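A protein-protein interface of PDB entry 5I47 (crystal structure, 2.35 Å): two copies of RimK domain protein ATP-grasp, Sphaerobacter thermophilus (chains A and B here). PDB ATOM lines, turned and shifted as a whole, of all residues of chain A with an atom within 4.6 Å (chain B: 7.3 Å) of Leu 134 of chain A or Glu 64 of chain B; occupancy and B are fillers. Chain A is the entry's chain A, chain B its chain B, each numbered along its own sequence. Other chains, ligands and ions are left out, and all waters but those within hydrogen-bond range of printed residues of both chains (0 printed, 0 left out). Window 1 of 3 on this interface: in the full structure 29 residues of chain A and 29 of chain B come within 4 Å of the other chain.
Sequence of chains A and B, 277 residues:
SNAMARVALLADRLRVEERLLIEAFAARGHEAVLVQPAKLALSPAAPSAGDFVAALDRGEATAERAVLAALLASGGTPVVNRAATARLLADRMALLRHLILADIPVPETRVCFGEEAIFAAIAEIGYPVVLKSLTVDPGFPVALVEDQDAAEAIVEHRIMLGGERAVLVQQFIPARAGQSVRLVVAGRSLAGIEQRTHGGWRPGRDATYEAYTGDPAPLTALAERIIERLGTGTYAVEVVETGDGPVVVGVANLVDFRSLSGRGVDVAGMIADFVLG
The side-chain carboxylate (OD1) of Asp 91 of chain A lies within hydrogen-bond range of the backbone NH (N) of Met 93 of chain A. The backbone NH (N) of Arg 92 of chain A sits at hydrogen-bond distance from the backbone carbonyl oxygen (O) of Leu 134 of chain A (2.9 Å). The backbone carbonyl oxygen of Leu 134 of chain A sits at hydrogen-bond distance from the backbone NH of Met 93 of chain A (3.4 Å). The side-chain hydroxyl (OG1) of Thr 62 of chain B sits at hydrogen-bond distance from the side-chain carboxylate (OE1) of Glu 64 of chain B.
Among the printed residues, merely in contact across the chains: Met 93 of chain A with Val 67 of chain B (3.99 Å), Met 93 of chain A with Leu 71 of chain B (3.9 Å), Val 111 of chain A with Leu 71 of chain B (3.8 Å), Phe 113 of chain A with Glu 64 of chain B (3.3 Å), Phe 113 of chain A with Leu 68 of chain B (3.7 Å), Phe 113 of chain A with Leu 71 of chain B (3.9 Å), Leu 134 of chain A with Glu 64 of chain B (3.8 Å), Arg 165 of chain A with Glu 64 of chain B (3.7 Å) and Ala 166 of chain A with Glu 64 of chain B (3.6 Å).
Leu 134 of chain A touches just one residue of chain B: Glu 64. Of the printed residues of chain B, Arg 165 of chain A touches Glu 64. Of the printed residues of chain A, Glu 64 of chain B touches Phe 113, Leu 134, Arg 165 and Ala 166. Printed residues of chain A within 4 Å of Leu 68 of chain B: Phe 113. Printed residues of chain A within 4 Å of Leu 71 of chain B: Met 93 (3.9 Å), Val 111 (3.8 Å) and Phe 113 (3.9 Å).
Of the 16 printed residues of chain B, 4 touch a printed residue of chain A. Printed residues of chain A that touch a printed residue of chain B: Met 93, Val 111, Phe 113, Leu 134, Arg 165 and Ala 166. Hydrophobic or aromatic side chains of chain A within 4 Å of the printed part of chain B: Met 93, Val 111, Phe 113, Leu 134 and Ala 166. Among the printed residues, 9 pairs touch across the chains. Among the printed residues, no Asp or Glu carboxylate lies within 4 Å of a Lys or Arg side-chain nitrogen of the other chain.
Positions printed for both chains: 90, 135 and 136. Of the 9 pairs that touch across the chains among the printed residues, none has its exchanged pair printed and touching as well.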
ATOM      1  N   ALA A  90      31.981  -1.294 -24.533  1.00  0.00           N
ATOM      2  CA  ALA A  90      30.815  -1.913 -23.910  1.00  0.00           C
ATOM      3  C   ALA A  90      29.517  -1.194 -24.225  1.00  0.00           C
ATOM      4  O   ALA A  90      28.460  -1.832 -24.280  1.00  0.00           O
ATOM      5  CB  ALA A  90      30.990  -1.963 -22.390  1.00  0.00           C
ATOM      6  N   ASP A  91      29.567   0.115 -24.425  1.00  0.00           N
ATOM      7  CA  ASP A  91      28.375   0.941 -24.558  1.00  0.00           C
ATOM      8  C   ASP A  91      28.179   1.245 -26.037  1.00  0.00           C
ATOM      9  O   ASP A  91      28.772   2.188 -26.570  1.00  0.00           O
ATOM     10  CB  ASP A  91      28.528   2.209 -23.725  1.00  0.00           C
ATOM     11  CG  ASP A  91      27.226   2.941 -23.525  1.00  0.00           C
ATOM     12  OD1 ASP A  91      26.353   2.848 -24.409  1.00  0.00           O
ATOM     13  OD2 ASP A  91      27.084   3.621 -22.482  1.00  0.00           O
ATOM     14  N   ARG A  92      27.334   0.443 -26.697  1.00  0.00           N
ATOM     15  CA  ARG A  92      27.039   0.662 -28.113  1.00  0.00           C
ATOM     16  C   ARG A  92      26.433   2.037 -28.358  1.00  0.00           C
ATOM     17  O   ARG A  92      26.646   2.627 -29.424  1.00  0.00           O
ATOM     18  CB  ARG A  92      26.090  -0.418 -28.637  1.00  0.00           C
ATOM     19  CG  ARG A  92      26.654  -1.826 -28.653  1.00  0.00           C
ATOM     20  CD  ARG A  92      25.795  -2.742 -29.516  1.00  0.00           C
ATOM     21  NE  ARG A  92      26.272  -4.123 -29.496  1.00  0.00           N
ATOM     22  CZ  ARG A  92      25.759  -5.076 -28.724  1.00  0.00           C
ATOM     23  NH1 ARG A  92      24.746  -4.800 -27.912  1.00  0.00           N
ATOM     24  NH2 ARG A  92      26.252  -6.304 -28.767  1.00  0.00           N
ATOM     25  N   MET A  93      25.671   2.553 -27.399  1.00  0.00           N
ATOM     26  CA  MET A  93      25.065   3.874 -27.516  1.00  0.00           C
ATOM     27  C   MET A  93      26.129   4.957 -27.467  1.00  0.00           C
ATOM     28  O   MET A  93      26.154   5.862 -28.301  1.00  0.00           O
ATOM     29  CB  MET A  93      24.039   4.103 -26.405  1.00  0.00           C
ATOM     30  CG  MET A  93      23.428   5.497 -26.408  1.00  0.00           C
ATOM     31  SD  MET A  93      22.371   5.866 -28.014  1.00  0.00           S
ATOM     32  CE  MET A  93      23.408   7.332 -28.789  1.00  0.00           C
ATOM     33  N   VAL A 111      17.253   4.722 -31.841  1.00  0.00           N
ATOM     34  CA  VAL A 111      17.224   4.305 -30.444  1.00  0.00           C
ATOM     35  C   VAL A 111      15.761   4.141 -30.046  1.00  0.00           C
ATOM     36  O   VAL A 111      15.013   5.118 -29.983  1.00  0.00           O
ATOM     37  CB  VAL A 111      17.943   5.312 -29.538  1.00  0.00           C
ATOM     38  CG1 VAL A 111      18.297   4.666 -28.206  1.00  0.00           C
ATOM     39  CG2 VAL A 111      19.184   5.860 -30.227  1.00  0.00           C
ATOM     40  N   PHE A 113      12.824   2.738 -27.381  1.00  0.00           N
ATOM     41  CA  PHE A 113      12.630   2.507 -25.956  1.00  0.00           C
ATOM     42  C   PHE A 113      11.373   1.696 -25.659  1.00  0.00           C
ATOM     43  O   PHE A 113      10.863   1.740 -24.536  1.00  0.00           O
ATOM     44  CB  PHE A 113      12.601   3.843 -25.209  1.00  0.00           C
ATOM     45  CG  PHE A 113      13.898   4.602 -25.286  1.00  0.00           C
ATOM     46  CD1 PHE A 113      14.156   5.455 -26.348  1.00  0.00           C
ATOM     47  CD2 PHE A 113      14.866   4.449 -24.305  1.00  0.00           C
ATOM     48  CE1 PHE A 113      15.349   6.144 -26.426  1.00  0.00           C
ATOM     49  CE2 PHE A 113      16.061   5.135 -24.378  1.00  0.00           C
ATOM     50  CZ  PHE A 113      16.304   5.982 -25.441  1.00  0.00           C
ATOM     51  N   LYS A 132      20.334  -4.558 -31.496  1.00  0.00           N
ATOM     52  CA  LYS A 132      21.478  -4.504 -30.598  1.00  0.00           C
ATOM     53  C   LYS A 132      21.051  -3.905 -29.268  1.00  0.00           C
ATOM     54  O   LYS A 132      20.482  -2.808 -29.232  1.00  0.00           O
ATOM     55  CB  LYS A 132      22.608  -3.665 -31.197  1.00  0.00           C
ATOM     56  CG  LYS A 132      23.243  -4.234 -32.443  1.00  0.00           C
ATOM     57  CD  LYS A 132      24.283  -3.269 -32.988  1.00  0.00           C
ATOM     58  CE  LYS A 132      25.054  -3.881 -34.136  1.00  0.00           C
ATOM     59  NZ  LYS A 132      25.942  -2.877 -34.780  1.00  0.00           N
ATOM     60  N   SER A 133      21.330  -4.618 -28.180  1.00  0.00           N
ATOM     61  CA  SER A 133      21.137  -4.052 -26.853  1.00  0.00           C
ATOM     62  C   SER A 133      22.051  -2.846 -26.665  1.00  0.00           C
ATOM     63  O   SER A 133      23.122  -2.753 -27.269  1.00  0.00           O
ATOM     64  CB  SER A 133      21.418  -5.102 -25.782  1.00  0.00           C
ATOM     65  OG  SER A 133      22.715  -5.644 -25.948  1.00  0.00           O
ATOM     66  N   LEU A 134      21.619  -1.913 -25.812  1.00  0.00           N
ATOM     67  CA  LEU A 134      22.354  -0.662 -25.651  1.00  0.00           C
ATOM     68  C   LEU A 134      23.788  -0.906 -25.188  1.00  0.00           C
ATOM     69  O   LEU A 134      24.716  -0.235 -25.653  1.00  0.00           O
ATOM     70  CB  LEU A 134      21.624   0.258 -24.677  1.00  0.00           C
ATOM     71  CG  LEU A 134      20.334   0.874 -25.216  1.00  0.00           C
ATOM     72  CD1 LEU A 134      19.717   1.806 -24.179  1.00  0.00           C
ATOM     73  CD2 LEU A 134      20.598   1.613 -26.524  1.00  0.00           C
ATOM     74  N   THR A 135      23.988  -1.855 -24.276  1.00  0.00           N
ATOM     75  CA  THR A 135      25.322  -2.248 -23.843  1.00  0.00           C
ATOM     76  C   THR A 135      25.555  -3.712 -24.188  1.00  0.00           C
ATOM     77  O   THR A 135      24.611  -4.502 -24.283  1.00  0.00           O
ATOM     78  CB  THR A 135      25.531  -2.023 -22.338  1.00  0.00           C
ATOM     79  OG1 THR A 135      24.606  -2.823 -21.596  1.00  0.00           O
ATOM     80  CG2 THR A 135      25.327  -0.551 -21.978  1.00  0.00           C
ATOM     81  N   VAL A 136      26.826  -4.064 -24.389  1.00  0.00           N
ATOM     82  CA  VAL A 136      27.168  -5.413 -24.826  1.00  0.00           C
ATOM     83  C   VAL A 136      26.767  -6.407 -23.746  1.00  0.00           C
ATOM     84  O   VAL A 136      27.249  -6.346 -22.609  1.00  0.00           O
ATOM     85  CB  VAL A 136      28.660  -5.510 -25.161  1.00  0.00           C
ATOM     86  CG1 VAL A 136      29.044  -6.955 -25.454  1.00  0.00           C
ATOM     87  CG2 VAL A 136      28.990  -4.609 -26.346  1.00  0.00           C
ATOM     88  N   ARG A 165      14.149  -3.223 -22.004  1.00  0.00           N
ATOM     89  CA  ARG A 165      13.086  -2.695 -22.852  1.00  0.00           C
ATOM     90  C   ARG A 165      13.579  -1.506 -23.663  1.00  0.00           C
ATOM     91  O   ARG A 165      12.896  -0.484 -23.783  1.00  0.00           O
ATOM     92  CB  ARG A 165      11.863  -2.311 -22.021  1.00  0.00           C
ATOM     93  N   ALA A 166      14.776  -1.620 -24.234  1.00  0.00           N
ATOM     94  CA  ALA A 166      15.319  -0.583 -25.100  1.00  0.00           C
ATOM     95  C   ALA A 166      16.407  -1.204 -25.958  1.00  0.00           C
ATOM     96  O   ALA A 166      17.280  -1.904 -25.438  1.00  0.00           O
ATOM     97  CB  ALA A 166      15.875   0.592 -24.290  1.00  0.00           C
ATOM     98  N   VAL A 167      16.343  -0.968 -27.267  1.00  0.00           N
ATOM     99  CA  VAL A 167      17.299  -1.539 -28.202  1.00  0.00           C
ATOM    100  C   VAL A 167      17.633  -0.511 -29.269  1.00  0.00           C
ATOM    101  O   VAL A 167      16.861   0.408 -29.551  1.00  0.00           O
ATOM    102  CB  VAL A 167      16.788  -2.834 -28.883  1.00  0.00           C
ATOM    103  CG1 VAL A 167      16.618  -3.966 -27.868  1.00  0.00           C
ATOM    104  CG2 VAL A 167      15.497  -2.564 -29.641  1.00  0.00           C
ATOM    105  N   LEU A 168      18.810  -0.678 -29.857  1.00  0.00           N
ATOM    106  CA  LEU A 168      19.159  -0.009 -31.098  1.00  0.00           C
ATOM    107  C   LEU A 168      18.621  -0.833 -32.260  1.00  0.00           C
ATOM    108  O   LEU A 168      18.858  -2.044 -32.336  1.00  0.00           O
ATOM    109  CB  LEU A 168      20.674   0.159 -31.228  1.00  0.00           C
ATOM    110  CG  LEU A 168      21.396   1.056 -30.223  1.00  0.00           C
ATOM    111  CD1 LEU A 168      22.884   1.132 -30.545  1.00  0.00           C
ATOM    112  CD2 LEU A 168      20.775   2.442 -30.208  1.00  0.00           C
ATOM    113  N   ASP B  57      11.112  12.906 -16.261  1.00  0.00           N
ATOM    114  CA  ASP B  57      11.045  11.450 -16.223  1.00  0.00           C
ATOM    115  C   ASP B  57      10.291  11.018 -14.975  1.00  0.00           C
ATOM    116  O   ASP B  57      10.765  11.218 -13.851  1.00  0.00           O
ATOM    117  CB  ASP B  57      12.447  10.848 -16.256  1.00  0.00           C
ATOM    118  CG  ASP B  57      12.438   9.367 -16.584  1.00  0.00           C
ATOM    119  OD1 ASP B  57      11.473   8.672 -16.215  1.00  0.00           O
ATOM    120  OD2 ASP B  57      13.401   8.896 -17.217  1.00  0.00           O
ATOM    121  N   ALA B  61      14.144   4.685 -12.132  1.00  0.00           N
ATOM    122  CA  ALA B  61      15.462   4.989 -12.673  1.00  0.00           C
ATOM    123  C   ALA B  61      16.140   3.713 -13.155  1.00  0.00           C
ATOM    124  O   ALA B  61      16.376   2.794 -12.366  1.00  0.00           O
ATOM    125  CB  ALA B  61      16.315   5.680 -11.616  1.00  0.00           C
ATOM    126  N   THR B  62      16.464   3.658 -14.447  1.00  0.00           N
ATOM    127  CA  THR B  62      17.196   2.532 -15.014  1.00  0.00           C
ATOM    128  C   THR B  62      18.203   3.052 -16.033  1.00  0.00           C
ATOM    129  O   THR B  62      18.246   4.248 -16.340  1.00  0.00           O
ATOM    130  CB  THR B  62      16.258   1.514 -15.662  1.00  0.00           C
ATOM    131  OG1 THR B  62      17.030   0.401 -16.128  1.00  0.00           O
ATOM    132  CG2 THR B  62      15.537   2.141 -16.840  1.00  0.00           C
ATOM    133  N   ALA B  63      19.014   2.136 -16.567  1.00  0.00           N
ATOM    134  CA  ALA B  63      20.116   2.536 -17.433  1.00  0.00           C
ATOM    135  C   ALA B  63      19.618   3.214 -18.703  1.00  0.00           C
ATOM    136  O   ALA B  63      20.182   4.228 -19.130  1.00  0.00           O
ATOM    137  CB  ALA B  63      20.981   1.324 -17.780  1.00  0.00           C
ATOM    138  N   GLU B  64      18.561   2.678 -19.321  1.00  0.00           N
ATOM    139  CA  GLU B  64      18.107   3.248 -20.585  1.00  0.00           C
ATOM    140  C   GLU B  64      17.386   4.578 -20.402  1.00  0.00           C
ATOM    141  O   GLU B  64      17.289   5.354 -21.361  1.00  0.00           O
ATOM    142  CB  GLU B  64      17.204   2.265 -21.333  1.00  0.00           C
ATOM    143  CG  GLU B  64      16.020   1.759 -20.544  1.00  0.00           C
ATOM    144  CD  GLU B  64      16.293   0.420 -19.885  1.00  0.00           C
ATOM    145  OE1 GLU B  64      17.438   0.200 -19.424  1.00  0.00           O
ATOM    146  OE2 GLU B  64      15.362  -0.417 -19.839  1.00  0.00           O
ATOM    147  N   ARG B  65      16.881   4.870 -19.206  1.00  0.00           N
ATOM    148  CA  ARG B  65      16.277   6.181 -19.010  1.00  0.00           C
ATOM    149  C   ARG B  65      17.332   7.261 -18.821  1.00  0.00           C
ATOM    150  O   ARG B  65      17.099   8.415 -19.192  1.00  0.00           O
ATOM    151  CB  ARG B  65      15.300   6.137 -17.839  1.00  0.00           C
ATOM    152  CG  ARG B  65      14.173   5.145 -18.093  1.00  0.00           C
ATOM    153  CD  ARG B  65      13.034   5.324 -17.135  1.00  0.00           C
ATOM    154  NE  ARG B  65      12.087   6.347 -17.574  1.00  0.00           N
ATOM    155  CZ  ARG B  65      10.924   6.085 -18.163  1.00  0.00           C
ATOM    156  NH1 ARG B  65      10.565   4.831 -18.397  1.00  0.00           N
ATOM    157  NH2 ARG B  65      10.118   7.078 -18.513  1.00  0.00           N
ATOM    158  N   ALA B  66      18.496   6.910 -18.271  1.00  0.00           N
ATOM    159  CA  ALA B  66      19.634   7.819 -18.338  1.00  0.00           C
ATOM    160  C   ALA B  66      20.074   8.025 -19.780  1.00  0.00           C
ATOM    161  O   ALA B  66      20.430   9.141 -20.172  1.00  0.00           O
ATOM    162  CB  ALA B  66      20.791   7.290 -17.493  1.00  0.00           C
ATOM    163  N   VAL B  67      20.044   6.957 -20.583  1.00  0.00           N
ATOM    164  CA  VAL B  67      20.293   7.080 -22.020  1.00  0.00           C
ATOM    165  C   VAL B  67      19.266   8.005 -22.659  1.00  0.00           C
ATOM    166  O   VAL B  67      19.599   8.825 -23.524  1.00  0.00           O
ATOM    167  CB  VAL B  67      20.291   5.688 -22.683  1.00  0.00           C
ATOM    168  CG1 VAL B  67      20.129   5.811 -24.192  1.00  0.00           C
ATOM    169  CG2 VAL B  67      21.568   4.932 -22.347  1.00  0.00           C
ATOM    170  N   LEU B  68      18.001   7.888 -22.240  1.00  0.00           N
ATOM    171  CA  LEU B  68      16.946   8.722 -22.807  1.00  0.00           C
ATOM    172  C   LEU B  68      17.119  10.181 -22.407  1.00  0.00           C
ATOM    173  O   LEU B  68      16.915  11.083 -23.230  1.00  0.00           O
ATOM    174  CB  LEU B  68      15.576   8.203 -22.367  1.00  0.00           C
ATOM    175  CG  LEU B  68      14.359   9.041 -22.769  1.00  0.00           C
ATOM    176  CD1 LEU B  68      14.254   9.147 -24.281  1.00  0.00           C
ATOM    177  CD2 LEU B  68      13.088   8.454 -22.180  1.00  0.00           C
ATOM    178  N   ALA B  69      17.492  10.432 -21.148  1.00  0.00           N
ATOM    179  CA  ALA B  69      17.718  11.802 -20.698  1.00  0.00           C
ATOM    180  C   ALA B  69      18.900  12.436 -21.420  1.00  0.00           C
ATOM    181  O   ALA B  69      18.893  13.641 -21.697  1.00  0.00           O
ATOM    182  CB  ALA B  69      17.942  11.826 -19.188  1.00  0.00           C
ATOM    183  N   ALA B  70      19.929  11.643 -21.729  1.00  0.00           N
ATOM    184  CA  ALA B  70      21.098  12.194 -22.408  1.00  0.00           C
ATOM    185  C   ALA B  70      20.798  12.488 -23.870  1.00  0.00           C
ATOM    186  O   ALA B  70      21.247  13.505 -24.411  1.00  0.00           O
ATOM    187  CB  ALA B  70      22.280  11.232 -22.287  1.00  0.00           C
ATOM    188  N   LEU B  71      20.047  11.605 -24.528  1.00  0.00           N
ATOM    189  CA  LEU B  71      19.677  11.831 -25.921  1.00  0.00           C
ATOM    190  C   LEU B  71      18.802  13.066 -26.055  1.00  0.00           C
ATOM    191  O   LEU B  71      19.076  13.953 -26.873  1.00  0.00           O
ATOM    192  CB  LEU B  71      18.959  10.599 -26.476  1.00  0.00           C
ATOM    193  CG  LEU B  71      19.844   9.469 -26.984  1.00  0.00           C
ATOM    194  CD1 LEU B  71      19.049   8.184 -27.098  1.00  0.00           C
ATOM    195  CD2 LEU B  71      20.446   9.856 -28.326  1.00  0.00           C
ATOM    196  N   ALA B  90      20.543   5.164 -11.579  1.00  0.00           N
ATOM    197  CA  ALA B  90      20.485   3.895 -12.288  1.00  0.00           C
ATOM    198  C   ALA B  90      21.669   2.991 -11.992  1.00  0.00           C
ATOM    199  O   ALA B  90      21.550   1.769 -12.137  1.00  0.00           O
ATOM    200  CB  ALA B  90      20.416   4.142 -13.797  1.00  0.00           C
ATOM    201  N   THR B 135      23.675  -2.217 -11.722  1.00  0.00           N
ATOM    202  CA  THR B 135      22.686  -1.354 -12.348  1.00  0.00           C
ATOM    203  C   THR B 135      21.301  -1.757 -11.865  1.00  0.00           C
ATOM    204  O   THR B 135      20.995  -2.951 -11.773  1.00  0.00           O
ATOM    205  CB  THR B 135      22.770  -1.449 -13.876  1.00  0.00           C
ATOM    206  OG1 THR B 135      23.937  -0.749 -14.329  1.00  0.00           O
ATOM    207  CG2 THR B 135      21.528  -0.859 -14.538  1.00  0.00           C
ATOM    208  N   VAL B 136      20.475  -0.758 -11.536  1.00  0.00           N
ATOM    209  CA  VAL B 136      19.112  -1.032 -11.094  1.00  0.00           C
ATOM    210  C   VAL B 136      18.367  -1.764 -12.197  1.00  0.00           C
ATOM    211  O   VAL B 136      18.300  -1.302 -13.343  1.00  0.00           O
ATOM    212  CB  VAL B 136      18.395   0.269 -10.701  1.00  0.00           C
ATOM    213  CG1 VAL B 136      16.956  -0.025 -10.316  1.00  0.00           C
ATOM    214  CG2 VAL B 136      19.124   0.951  -9.553  1.00  0.00           C
ATOM    215  N   PRO B 138      14.834  -4.418 -12.731  1.00  0.00           N
ATOM    216  CA  PRO B 138      13.686  -5.127 -12.138  1.00  0.00           C
ATOM    217  C   PRO B 138      13.809  -6.640 -12.201  1.00  0.00           C
ATOM    218  O   PRO B 138      13.257  -7.332 -11.336  1.00  0.00           O
ATOM    219  CB  PRO B 138      12.494  -4.614 -12.960  1.00  0.00           C
ATOM    220  CG  PRO B 138      13.094  -4.096 -14.233  1.00  0.00           C
ATOM    221  CD  PRO B 138      14.446  -3.568 -13.868  1.00  0.00           C
